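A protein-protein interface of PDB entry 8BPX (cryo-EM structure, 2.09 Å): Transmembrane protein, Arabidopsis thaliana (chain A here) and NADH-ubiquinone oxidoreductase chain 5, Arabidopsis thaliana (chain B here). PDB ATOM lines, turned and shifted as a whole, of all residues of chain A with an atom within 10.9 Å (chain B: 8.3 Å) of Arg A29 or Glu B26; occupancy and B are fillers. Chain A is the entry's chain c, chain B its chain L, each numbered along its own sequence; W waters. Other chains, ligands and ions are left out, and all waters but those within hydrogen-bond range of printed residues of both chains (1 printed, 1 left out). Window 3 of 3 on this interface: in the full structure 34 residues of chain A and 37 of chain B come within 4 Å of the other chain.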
ATOM      1  N   SER A  21      34.672   7.499   4.459  1.00  0.00           N
ATOM      2  CA  SER A  21      33.959   8.769   4.398  1.00  0.00           C
ATOM      3  C   SER A  21      33.119   8.940   5.656  1.00  0.00           C
ATOM      4  O   SER A  21      32.791   7.975   6.348  1.00  0.00           O
ATOM      5  CB  SER A  21      33.063   8.887   3.153  1.00  0.00           C
ATOM      6  OG  SER A  21      32.175   7.798   3.037  1.00  0.00           O
ATOM      7  N   THR A  23      29.995  10.145   5.667  1.00  0.00           N
ATOM      8  CA  THR A  23      28.620   9.763   5.377  1.00  0.00           C
ATOM      9  C   THR A  23      28.476   8.267   5.127  1.00  0.00           C
ATOM     10  O   THR A  23      27.348   7.771   5.054  1.00  0.00           O
ATOM     11  CB  THR A  23      28.103  10.567   4.181  1.00  0.00           C
ATOM     12  OG1 THR A  23      28.587  11.912   4.276  1.00  0.00           O
ATOM     13  CG2 THR A  23      26.584  10.621   4.173  1.00  0.00           C
ATOM     14  N   GLY A  24      29.585   7.539   5.008  1.00  0.00           N
ATOM     15  CA  GLY A  24      29.561   6.096   4.964  1.00  0.00           C
ATOM     16  C   GLY A  24      29.749   5.467   3.601  1.00  0.00           C
ATOM     17  O   GLY A  24      29.912   4.247   3.530  1.00  0.00           O
ATOM     18  N   GLY A  25      29.722   6.241   2.523  1.00  0.00           N
ATOM     19  CA  GLY A  25      29.905   5.690   1.201  1.00  0.00           C
ATOM     20  C   GLY A  25      28.696   4.924   0.698  1.00  0.00           C
ATOM     21  O   GLY A  25      27.612   4.984   1.278  1.00  0.00           O
ATOM     22  N   PRO A  26      28.867   4.177  -0.391  1.00  0.00           N
ATOM     23  CA  PRO A  26      27.720   3.527  -1.036  1.00  0.00           C
ATOM     24  C   PRO A  26      27.225   2.292  -0.294  1.00  0.00           C
ATOM     25  O   PRO A  26      28.010   1.446   0.141  1.00  0.00           O
ATOM     26  CB  PRO A  26      28.267   3.151  -2.418  1.00  0.00           C
ATOM     27  CG  PRO A  26      29.730   2.974  -2.194  1.00  0.00           C
ATOM     28  CD  PRO A  26      30.122   3.949  -1.129  1.00  0.00           C
ATOM     29  N   ASN A  27      25.897   2.193  -0.177  1.00  0.00           N
ATOM     30  CA  ASN A  27      25.221   1.021   0.388  1.00  0.00           C
ATOM     31  C   ASN A  27      25.699   0.727   1.809  1.00  0.00           C
ATOM     32  O   ASN A  27      26.063  -0.396   2.146  1.00  0.00           O
ATOM     33  CB  ASN A  27      25.405  -0.202  -0.514  1.00  0.00           C
ATOM     34  CG  ASN A  27      24.786  -0.017  -1.883  1.00  0.00           C
ATOM     35  OD1 ASN A  27      23.597   0.256  -2.006  1.00  0.00           O
ATOM     36  ND2 ASN A  27      25.601  -0.137  -2.920  1.00  0.00           N
ATOM     37  N   CYS A  28      25.696   1.759   2.647  1.00  0.00           N
ATOM     38  CA  CYS A  28      26.217   1.648   4.004  1.00  0.00           C
ATOM     39  C   CYS A  28      25.197   0.952   4.905  1.00  0.00           C
ATOM     40  O   CYS A  28      24.079   1.444   5.085  1.00  0.00           O
ATOM     41  CB  CYS A  28      26.573   3.030   4.544  1.00  0.00           C
ATOM     42  SG  CYS A  28      27.357   3.024   6.165  1.00  0.00           S
ATOM     43  N   ARG A  29      25.594  -0.185   5.471  1.00  0.00           N
ATOM     44  CA  ARG A  29      24.740  -1.018   6.321  1.00  0.00           C
ATOM     45  C   ARG A  29      25.486  -1.381   7.597  1.00  0.00           C
ATOM     46  O   ARG A  29      25.865  -2.541   7.789  1.00  0.00           O
ATOM     47  CB  ARG A  29      24.343  -2.298   5.586  1.00  0.00           C
ATOM     48  CG  ARG A  29      23.533  -2.110   4.325  1.00  0.00           C
ATOM     49  CD  ARG A  29      22.078  -1.853   4.631  1.00  0.00           C
ATOM     50  NE  ARG A  29      21.573  -2.891   5.519  1.00  0.00           N
ATOM     51  CZ  ARG A  29      20.327  -2.968   5.959  1.00  0.00           C
ATOM     52  NH1 ARG A  29      19.379  -2.187   5.476  1.00  0.00           N
ATOM     53  NH2 ARG A  29      20.017  -3.882   6.871  1.00  0.00           N
ATOM     54  N   PRO A  30      25.714  -0.423   8.496  1.00  0.00           N
ATOM     55  CA  PRO A  30      26.400  -0.755   9.752  1.00  0.00           C
ATOM     56  C   PRO A  30      25.614  -1.783  10.556  1.00  0.00           C
ATOM     57  O   PRO A  30      24.383  -1.753  10.607  1.00  0.00           O
ATOM     58  CB  PRO A  30      26.494   0.593  10.478  1.00  0.00           C
ATOM     59  CG  PRO A  30      25.503   1.465   9.813  1.00  0.00           C
ATOM     60  CD  PRO A  30      25.387   1.007   8.407  1.00  0.00           C
ATOM     61  N   LYS A  31      26.348  -2.702  11.187  1.00  0.00           N
ATOM     62  CA  LYS A  31      25.715  -3.830  11.862  1.00  0.00           C
ATOM     63  C   LYS A  31      24.880  -3.376  13.053  1.00  0.00           C
ATOM     64  O   LYS A  31      23.795  -3.912  13.300  1.00  0.00           O
ATOM     65  CB  LYS A  31      26.776  -4.841  12.300  1.00  0.00           C
ATOM     66  CG  LYS A  31      26.316  -5.800  13.375  1.00  0.00           C
ATOM     67  CD  LYS A  31      27.467  -6.213  14.273  1.00  0.00           C
ATOM     68  CE  LYS A  31      27.709  -7.714  14.203  1.00  0.00           C
ATOM     69  NZ  LYS A  31      28.467  -8.219  15.382  1.00  0.00           N
ATOM     70  N   HIS A  32      25.362  -2.382  13.791  1.00  0.00           N
ATOM     71  CA  HIS A  32      24.687  -1.890  14.990  1.00  0.00           C
ATOM     72  C   HIS A  32      23.932  -0.597  14.730  1.00  0.00           C
ATOM     73  O   HIS A  32      23.871   0.277  15.595  1.00  0.00           O
ATOM     74  CB  HIS A  32      25.695  -1.705  16.113  1.00  0.00           C
ATOM     75  CG  HIS A  32      26.325  -2.984  16.566  1.00  0.00           C
ATOM     76  ND1 HIS A  32      25.582  -4.063  16.993  1.00  0.00           N
ATOM     77  CD2 HIS A  32      27.622  -3.360  16.648  1.00  0.00           C
ATOM     78  CE1 HIS A  32      26.398  -5.047  17.327  1.00  0.00           C
ATOM     79  NE2 HIS A  32      27.641  -4.644  17.130  1.00  0.00           N
ATOM     80  N   TRP A  33      23.331  -0.460  13.546  1.00  0.00           N
ATOM     81  CA  TRP A  33      22.758   0.823  13.160  1.00  0.00           C
ATOM     82  C   TRP A  33      21.556   1.206  14.018  1.00  0.00           C
ATOM     83  O   TRP A  33      21.290   2.396  14.191  1.00  0.00           O
ATOM     84  CB  TRP A  33      22.382   0.815  11.675  1.00  0.00           C
ATOM     85  CG  TRP A  33      21.189  -0.014  11.338  1.00  0.00           C
ATOM     86  CD1 TRP A  33      21.183  -1.305  10.911  1.00  0.00           C
ATOM     87  CD2 TRP A  33      19.819   0.399  11.386  1.00  0.00           C
ATOM     88  NE1 TRP A  33      19.898  -1.727  10.695  1.00  0.00           N
ATOM     89  CE2 TRP A  33      19.039  -0.700  10.978  1.00  0.00           C
ATOM     90  CE3 TRP A  33      19.176   1.589  11.736  1.00  0.00           C
ATOM     91  CZ2 TRP A  33      17.650  -0.646  10.912  1.00  0.00           C
ATOM     92  CZ3 TRP A  33      17.797   1.642  11.668  1.00  0.00           C
ATOM     93  CH2 TRP A  33      17.049   0.533  11.260  1.00  0.00           C
ATOM     94  N   ARG A  34      20.821   0.232  14.563  1.00  0.00           N
ATOM     95  CA  ARG A  34      19.687   0.560  15.428  1.00  0.00           C
ATOM     96  C   ARG A  34      20.139   1.201  16.732  1.00  0.00           C
ATOM     97  O   ARG A  34      19.619   2.251  17.132  1.00  0.00           O
ATOM     98  CB  ARG A  34      18.852  -0.684  15.717  1.00  0.00           C
ATOM     99  CG  ARG A  34      17.856  -0.998  14.640  1.00  0.00           C
ATOM    100  CD  ARG A  34      17.541  -2.458  14.597  1.00  0.00           C
ATOM    101  NE  ARG A  34      17.584  -2.923  13.223  1.00  0.00           N
ATOM    102  CZ  ARG A  34      17.907  -4.153  12.855  1.00  0.00           C
ATOM    103  NH1 ARG A  34      18.190  -5.089  13.745  1.00  0.00           N
ATOM    104  NH2 ARG A  34      17.945  -4.447  11.562  1.00  0.00           N
ATOM    105  N   ARG A  35      21.098   0.576  17.417  1.00  0.00           N
ATOM    106  CA  ARG A  35      21.609   1.149  18.654  1.00  0.00           C
ATOM    107  C   ARG A  35      22.279   2.495  18.391  1.00  0.00           C
ATOM    108  O   ARG A  35      22.145   3.432  19.185  1.00  0.00           O
ATOM    109  CB  ARG A  35      22.573   0.167  19.321  1.00  0.00           C
ATOM    110  CG  ARG A  35      23.580   0.807  20.255  1.00  0.00           C
ATOM    111  CD  ARG A  35      24.863   0.014  20.312  1.00  0.00           C
ATOM    112  NE  ARG A  35      25.851   0.528  19.373  1.00  0.00           N
ATOM    113  CZ  ARG A  35      26.979  -0.092  19.057  1.00  0.00           C
ATOM    114  NH1 ARG A  35      27.303  -1.254  19.597  1.00  0.00           N
ATOM    115  NH2 ARG A  35      27.799   0.466  18.172  1.00  0.00           N
ATOM    116  N   ASN A  36      22.979   2.616  17.262  1.00  0.00           N
ATOM    117  CA  ASN A  36      23.605   3.887  16.914  1.00  0.00           C
ATOM    118  C   ASN A  36      22.564   4.967  16.644  1.00  0.00           C
ATOM    119  O   ASN A  36      22.749   6.125  17.031  1.00  0.00           O
ATOM    120  CB  ASN A  36      24.529   3.693  15.715  1.00  0.00           C
ATOM    121  CG  ASN A  36      25.699   2.786  16.033  1.00  0.00           C
ATOM    122  OD1 ASN A  36      26.037   2.589  17.196  1.00  0.00           O
ATOM    123  ND2 ASN A  36      26.319   2.230  15.007  1.00  0.00           N
ATOM    124  N   THR A  37      21.454   4.571  16.036  1.00  0.00           N
ATOM    125  CA  THR A  37      20.357   5.507  15.742  1.00  0.00           C
ATOM    126  C   THR A  37      19.752   5.989  17.063  1.00  0.00           C
ATOM    127  O   THR A  37      19.598   7.172  17.201  1.00  0.00           O
ATOM    128  CB  THR A  37      19.410   4.927  14.685  1.00  0.00           C
ATOM    129  OG1 THR A  37      20.161   4.737  13.495  1.00  0.00           O
ATOM    130  CG2 THR A  37      18.240   5.841  14.392  1.00  0.00           C
ATOM    131  N   ALA A  38      19.555   5.069  18.008  1.00  0.00           N
ATOM    132  CA  ALA A  38      19.030   5.426  19.323  1.00  0.00           C
ATOM    133  C   ALA A  38      19.974   6.375  20.058  1.00  0.00           C
ATOM    134  O   ALA A  38      19.531   7.355  20.676  1.00  0.00           O
ATOM    135  CB  ALA A  38      18.781   4.163  20.146  1.00  0.00           C
ATOM    136  N   ALA A  40      22.072   8.450  18.681  1.00  0.00           N
ATOM    137  CA  ALA A  40      22.001   9.761  17.974  1.00  0.00           C
ATOM    138  C   ALA A  40      20.756  10.553  18.398  1.00  0.00           C
ATOM    139  O   ALA A  40      20.855  11.725  18.522  1.00  0.00           O
ATOM    140  CB  ALA A  40      22.059   9.608  16.472  1.00  0.00           C
ATOM    141  N   MET A  41      19.643   9.855  18.578  1.00  0.00           N
ATOM    142  CA  MET A  41      18.361  10.476  18.984  1.00  0.00           C
ATOM    143  C   MET A  41      18.490  10.988  20.408  1.00  0.00           C
ATOM    144  O   MET A  41      18.170  12.130  20.587  1.00  0.00           O
ATOM    145  CB  MET A  41      17.215   9.492  18.821  1.00  0.00           C
ATOM    146  CG  MET A  41      16.910   9.154  17.405  1.00  0.00           C
ATOM    147  SD  MET A  41      15.606   7.925  17.347  1.00  0.00           S
ATOM    148  CE  MET A  41      14.204   8.927  17.836  1.00  0.00           C
ATOM    149  N   GLY B  20      26.882   9.629   9.347  1.00  0.00           N
ATOM    150  CA  GLY B  20      26.141   8.713   8.505  1.00  0.00           C
ATOM    151  C   GLY B  20      26.770   7.342   8.383  1.00  0.00           C
ATOM    152  O   GLY B  20      26.063   6.373   8.106  1.00  0.00           O
ATOM    153  N   ARG B  21      28.083   7.234   8.599  1.00  0.00           N
ATOM    154  CA  ARG B  21      28.741   5.935   8.555  1.00  0.00           C
ATOM    155  C   ARG B  21      28.328   5.032   9.713  1.00  0.00           C
ATOM    156  O   ARG B  21      28.491   3.814   9.617  1.00  0.00           O
ATOM    157  CB  ARG B  21      30.263   6.116   8.550  1.00  0.00           C
ATOM    158  CG  ARG B  21      30.807   6.722   9.827  1.00  0.00           C
ATOM    159  CD  ARG B  21      32.309   6.922   9.768  1.00  0.00           C
ATOM    160  NE  ARG B  21      32.822   7.574  10.966  1.00  0.00           N
ATOM    161  CZ  ARG B  21      32.752   8.876  11.206  1.00  0.00           C
ATOM    162  NH1 ARG B  21      32.151   9.700  10.363  1.00  0.00           N
ATOM    163  NH2 ARG B  21      33.299   9.364  12.315  1.00  0.00           N
ATOM    164  N   PHE B  22      27.804   5.596  10.803  1.00  0.00           N
ATOM    165  CA  PHE B  22      27.332   4.797  11.925  1.00  0.00           C
ATOM    166  C   PHE B  22      25.850   4.462  11.841  1.00  0.00           C
ATOM    167  O   PHE B  22      25.411   3.495  12.471  1.00  0.00           O
ATOM    168  CB  PHE B  22      27.610   5.519  13.248  1.00  0.00           C
ATOM    169  CG  PHE B  22      29.051   5.860  13.461  1.00  0.00           C
ATOM    170  CD1 PHE B  22      29.997   4.859  13.608  1.00  0.00           C
ATOM    171  CD2 PHE B  22      29.468   7.179  13.501  1.00  0.00           C
ATOM    172  CE1 PHE B  22      31.332   5.170  13.801  1.00  0.00           C
ATOM    173  CE2 PHE B  22      30.800   7.493  13.695  1.00  0.00           C
ATOM    174  CZ  PHE B  22      31.731   6.485  13.843  1.00  0.00           C
ATOM    175  N   LEU B  23      25.084   5.192  11.076  1.00  0.00           N
ATOM    176  CA  LEU B  23      23.610   5.054  10.951  1.00  0.00           C
ATOM    177  C   LEU B  23      23.219   4.328   9.695  1.00  0.00           C
ATOM    178  O   LEU B  23      22.198   3.679   9.751  1.00  0.00           O
ATOM    179  CB  LEU B  23      22.975   6.440  10.945  1.00  0.00           C
ATOM    180  CG  LEU B  23      22.561   6.999  12.309  1.00  0.00           C
ATOM    181  CD1 LEU B  23      23.697   7.029  13.313  1.00  0.00           C
ATOM    182  CD2 LEU B  23      21.951   8.377  12.160  1.00  0.00           C
ATOM    183  N   GLY B  24      24.023   4.426   8.640  1.00  0.00           N
ATOM    184  CA  GLY B  24      23.628   3.901   7.368  1.00  0.00           C
ATOM    185  C   GLY B  24      22.369   4.549   6.818  1.00  0.00           C
ATOM    186  O   GLY B  24      21.857   5.555   7.313  1.00  0.00           O
ATOM    187  N   SER B  25      21.870   3.914   5.760  1.00  0.00           N
ATOM    188  CA  SER B  25      20.692   4.427   5.068  1.00  0.00           C
ATOM    189  C   SER B  25      19.514   4.553   6.019  1.00  0.00           C
ATOM    190  O   SER B  25      18.890   5.618   6.123  1.00  0.00           O
ATOM    191  CB  SER B  25      20.339   3.502   3.905  1.00  0.00           C
ATOM    192  OG  SER B  25      21.453   3.292   3.070  1.00  0.00           O
ATOM    193  N   GLU B  26      19.217   3.475   6.746  1.00  0.00           N
ATOM    194  CA  GLU B  26      18.029   3.435   7.589  1.00  0.00           C
ATOM    195  C   GLU B  26      18.102   4.456   8.711  1.00  0.00           C
ATOM    196  O   GLU B  26      17.160   5.236   8.912  1.00  0.00           O
ATOM    197  CB  GLU B  26      17.847   2.029   8.152  1.00  0.00           C
ATOM    198  CG  GLU B  26      17.217   1.083   7.175  1.00  0.00           C
ATOM    199  CD  GLU B  26      18.217   0.485   6.238  1.00  0.00           C
ATOM    200  OE1 GLU B  26      19.071  -0.291   6.705  1.00  0.00           O
ATOM    201  OE2 GLU B  26      18.156   0.807   5.034  1.00  0.00           O
ATOM    202  N   GLY B  27      19.173   4.434   9.490  1.00  0.00           N
ATOM    203  CA  GLY B  27      19.346   5.419  10.562  1.00  0.00           C
ATOM    204  C   GLY B  27      19.227   6.846  10.111  1.00  0.00           C
ATOM    205  O   GLY B  27      18.493   7.570  10.762  1.00  0.00           O
ATOM    206  N   SER B  28      19.893   7.215   9.025  1.00  0.00           N
ATOM    207  CA  SER B  28      19.953   8.577   8.482  1.00  0.00           C
ATOM    208  C   SER B  28      18.562   8.990   7.956  1.00  0.00           C
ATOM    209  O   SER B  28      18.170  10.112   8.238  1.00  0.00           O
ATOM    210  CB  SER B  28      21.121   8.724   7.475  1.00  0.00           C
ATOM    211  OG  SER B  28      22.383   8.467   8.059  1.00  0.00           O
ATOM    212  N   ALA B  29      17.818   8.047   7.409  1.00  0.00           N
ATOM    213  CA  ALA B  29      16.445   8.287   6.918  1.00  0.00           C
ATOM    214  C   ALA B  29      15.549   8.667   8.119  1.00  0.00           C
ATOM    215  O   ALA B  29      15.023   9.754   8.081  1.00  0.00           O
ATOM    216  CB  ALA B  29      15.992   7.111   6.143  1.00  0.00           C
ATOM    217  N   ILE B  30      15.648   7.910   9.185  1.00  0.00           N
ATOM    218  CA  ILE B  30      14.905   8.112  10.439  1.00  0.00           C
ATOM    219  C   ILE B  30      15.337   9.391  11.132  1.00  0.00           C
ATOM    220  O   ILE B  30      14.468  10.179  11.436  1.00  0.00           O
ATOM    221  CB  ILE B  30      15.087   6.876  11.346  1.00  0.00           C
ATOM    222  CG1 ILE B  30      14.411   5.645  10.740  1.00  0.00           C
ATOM    223  CG2 ILE B  30      14.586   7.154  12.751  1.00  0.00           C
ATOM    224  CD1 ILE B  30      14.430   4.419  11.609  1.00  0.00           C
ATOM    225  N   MET B  31      16.630   9.576  11.301  1.00  0.00           N
ATOM    226  CA  MET B  31      17.129  10.704  12.070  1.00  0.00           C
ATOM    227  C   MET B  31      16.642  11.986  11.411  1.00  0.00           C
ATOM    228  O   MET B  31      16.147  12.853  12.163  1.00  0.00           O
ATOM    229  CB  MET B  31      18.661  10.688  12.119  1.00  0.00           C
ATOM    230  CG  MET B  31      19.249  11.160  13.388  1.00  0.00           C
ATOM    231  SD  MET B  31      18.594  10.287  14.807  1.00  0.00           S
ATOM    232  CE  MET B  31      18.350  11.747  15.814  1.00  0.00           C
ATOM    233  N   THR B  32      16.824  12.083  10.101  1.00  0.00           N
ATOM    234  CA  THR B  32      16.515  13.323   9.374  1.00  0.00           C
ATOM    235  C   THR B  32      15.000  13.548   9.332  1.00  0.00           C
ATOM    236  O   THR B  32      14.604  14.673   9.461  1.00  0.00           O
ATOM    237  CB  THR B  32      17.250  13.422   8.024  1.00  0.00           C
ATOM    238  OG1 THR B  32      16.784  12.451   7.087  1.00  0.00           O
ATOM    239  CG2 THR B  32      18.757  13.371   8.171  1.00  0.00           C
ATOM    240  N   THR B  33      14.226  12.495   9.132  1.00  0.00           N
ATOM    241  CA  THR B  33      12.756  12.616   8.993  1.00  0.00           C
ATOM    242  C   THR B  33      12.176  13.055  10.341  1.00  0.00           C
ATOM    243  O   THR B  33      11.446  14.016  10.319  1.00  0.00           O
ATOM    244  CB  THR B  33      12.158  11.393   8.274  1.00  0.00           C
ATOM    245  OG1 THR B  33      12.803  11.250   7.009  1.00  0.00           O
ATOM    246  CG2 THR B  33      10.665  11.503   8.052  1.00  0.00           C
ATOM    247  N   ILE B 101      12.463   8.405   1.783  1.00  0.00           N
ATOM    248  CA  ILE B 101      12.826   7.173   2.486  1.00  0.00           C
ATOM    249  C   ILE B 101      12.603   5.951   1.604  1.00  0.00           C
ATOM    250  O   ILE B 101      13.421   5.025   1.578  1.00  0.00           O
ATOM    251  CB  ILE B 101      12.046   7.061   3.810  1.00  0.00           C
ATOM    252  CG1 ILE B 101      12.674   7.956   4.874  1.00  0.00           C
ATOM    253  CG2 ILE B 101      11.996   5.618   4.290  1.00  0.00           C
ATOM    254  CD1 ILE B 101      11.964   7.912   6.202  1.00  0.00           C
ATOM    255  N   MET B 104      14.350   6.715  -2.629  1.00  0.00           N
ATOM    256  CA  MET B 104      15.789   6.564  -2.779  1.00  0.00           C
ATOM    257  C   MET B 104      16.299   5.294  -2.114  1.00  0.00           C
ATOM    258  O   MET B 104      17.498   5.178  -1.843  1.00  0.00           O
ATOM    259  CB  MET B 104      16.505   7.787  -2.203  1.00  0.00           C
ATOM    260  CG  MET B 104      16.161   9.103  -2.893  1.00  0.00           C
ATOM    261  SD  MET B 104      16.882   9.274  -4.537  1.00  0.00           S
ATOM    262  CE  MET B 104      18.563   9.742  -4.122  1.00  0.00           C
ATOM    263  N   SER B 105      15.407   4.335  -1.852  1.00  0.00           N
ATOM    264  CA  SER B 105      15.769   3.163  -1.066  1.00  0.00           C
ATOM    265  C   SER B 105      16.817   2.306  -1.762  1.00  0.00           C
ATOM    266  O   SER B 105      17.632   1.663  -1.094  1.00  0.00           O
ATOM    267  CB  SER B 105      14.521   2.335  -0.762  1.00  0.00           C
ATOM    268  OG  SER B 105      14.153   1.545  -1.873  1.00  0.00           O
ATOM    269  N   PRO B 108      22.576   4.173  -3.884  1.00  0.00           N
ATOM    270  CA  PRO B 108      23.740   3.883  -3.031  1.00  0.00           C
ATOM    271  C   PRO B 108      24.022   4.939  -1.971  1.00  0.00           C
ATOM    272  O   PRO B 108      24.611   4.603  -0.939  1.00  0.00           O
ATOM    273  CB  PRO B 108      24.899   3.782  -4.034  1.00  0.00           C
ATOM    274  CG  PRO B 108      24.267   3.599  -5.359  1.00  0.00           C
ATOM    275  CD  PRO B 108      22.941   4.277  -5.307  1.00  0.00           C
ATOM    276  N   SER B 110      21.968   7.300  -0.127  1.00  0.00           N
ATOM    277  CA  SER B 110      20.827   7.947   0.521  1.00  0.00           C
ATOM    278  C   SER B 110      21.182   8.812   1.734  1.00  0.00           C
ATOM    279  O   SER B 110      20.531   9.856   1.908  1.00  0.00           O
ATOM    280  CB  SER B 110      19.770   6.891   0.880  1.00  0.00           C
ATOM    281  OG  SER B 110      20.161   6.084   1.970  1.00  0.00           O
ATOM    282  N   PRO B 111      22.132   8.450   2.615  1.00  0.00           N
ATOM    283  CA  PRO B 111      22.420   9.346   3.753  1.00  0.00           C
ATOM    284  C   PRO B 111      22.867  10.745   3.351  1.00  0.00           C
ATOM    285  O   PRO B 111      22.417  11.730   3.955  1.00  0.00           O
ATOM    286  CB  PRO B 111      23.518   8.591   4.517  1.00  0.00           C
ATOM    287  CG  PRO B 111      23.337   7.181   4.133  1.00  0.00           C
ATOM    288  CD  PRO B 111      22.923   7.210   2.707  1.00  0.00           C
ATOM    289  N   MET B 114      19.729  12.649   2.243  1.00  0.00           N
ATOM    290  CA  MET B 114      18.899  13.111   3.354  1.00  0.00           C
ATOM    291  C   MET B 114      19.549  14.281   4.081  1.00  0.00           C
ATOM    292  O   MET B 114      18.864  15.237   4.477  1.00  0.00           O
ATOM    293  CB  MET B 114      18.624  11.963   4.327  1.00  0.00           C
ATOM    294  CG  MET B 114      17.898  10.785   3.716  1.00  0.00           C
ATOM    295  SD  MET B 114      16.381  11.241   2.856  1.00  0.00           S
ATOM    296  CE  MET B 114      15.189  11.197   4.192  1.00  0.00           C
HETATM  297  O   HOH W   1      24.641   4.294   1.763  1.00  0.00           O
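Ser A21 touches Arg B21.
Thr A23 touches Gly B20 (O to C, 3.4 Å).
Gly A25 touches Pro B108.
Gly B24 touches Cys A28 (CA to O, 3.4 Å).
Arg B21 touches Pro A30 (O to CG, 3.8 Å).
C of Leu B23 touches CG of Pro A30 (3.7 Å).
Leu B23 touches Trp A33 (O to CB, 3.5 Å).
Glu B26 touches Trp A33 (CB to CZ3, 3.5 Å).
CA of Gly B27 touches OG1 of Thr A37, 3.1 Å away.
Met B31 touches Met A41.
O of Phe B22 sits at hydrogen-bond distance from ND2 of Asn A36 (3.0 Å).
SG of Cys A28 is in hydrogen-bond range of O of Arg B21, at 3.7 Å.
OE2 of Glu B26 is in salt-bridge range of NH1 of Arg A29 (3.3 Å).
O of Pro B108 is in hydrogen-bond range of N of Asn A27, at 2.8 Å.
N of Ser B25 sits at hydrogen-bond distance from O of Cys A28 (3.4 Å).
The backbone NH (N) of Gly A25 sits at hydrogen-bond distance from the side-chain hydroxyl (OG) of Ser A21 (3.0 Å).
The backbone carbonyl oxygen (O) of His A32 sits close to the side-chain amide nitrogen (ND2) of Asn A36.
The side-chain hydroxyl (OG) of Ser A21 sits at hydrogen-bond distance from the backbone NH (N) of Gly A24 (3.3 Å).
The backbone carbonyl oxygen (O) of Trp A33 sits at hydrogen-bond distance from the side-chain hydroxyl (OG1) of Thr A37 (2.7 Å).
The side-chain hydroxyl (OG) of Ser B28 sits at hydrogen-bond distance from the backbone carbonyl oxygen (O) of Gly B24, 3.1 Å away.
OG of Ser B110 lies close to OG of Ser B25, at 3.3 Å.
Water W1 lies within hydrogen-bond range of O of Pro B108 (2.7 Å), N of Cys A28 (2.9 Å), O of Gly A25 (3.1 Å) and N of Asn A27 (3.1 Å).
Of the printed residues of chain B, Ser A21 touches Arg B21 (3.6 Å).
Printed residues of chain B within 4 Å of Gly A25: Pro B108.
Cys A28 touches just these residues of chain B: Arg B21, Gly B24 and Ser B25.
Arg A29 touches just one residue of chain B: Glu B26.
Of chain B, only Arg B21 (3.8 Å), Phe B22 (3.3 Å), Leu B23 (3.7 Å) and Gly B24 (3.5 Å) come within 4 Å of Pro A30.
Printed residues of chain B within 4 Å of Trp A33: Phe B22, Leu B23, Glu B26 and Gly B27.
Gly B24 touches just these residues of chain A: Cys A28 and Pro A30.
Of chain A, only Cys A28 (3.4 Å) comes within 4 Å of Ser B25.
Glu B26 touches just these residues of chain A: Arg A29 and Trp A33.
No residue of chain A comes within 4 Å of Ser B28.
No residue of chain A comes within 4 Å of Ala B29.
No residue of chain A comes within 4 Å of Ile B30.
Ile B101 touches none of the printed residues of chain A.
Printed residues of chain A within 4 Å of Pro B111: Thr A23 (3.7 Å).
Of the 21 printed residues of chain B, 11 touch a printed residue of chain A.
Printed residues of chain B that touch a printed residue of chain A: Gly B20, Arg B21, Phe B22, Leu B23, Gly B24, Ser B25, Glu B26, Gly B27, Met B31, Pro B108 and Pro B111.
Hydrophobic or aromatic side chains of chain B within 4 Å of the printed part of chain A: Phe B22, Leu B23, Met B31, Pro B108 and Pro B111.
Among the printed residues, 26 pairs touch across the chains.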
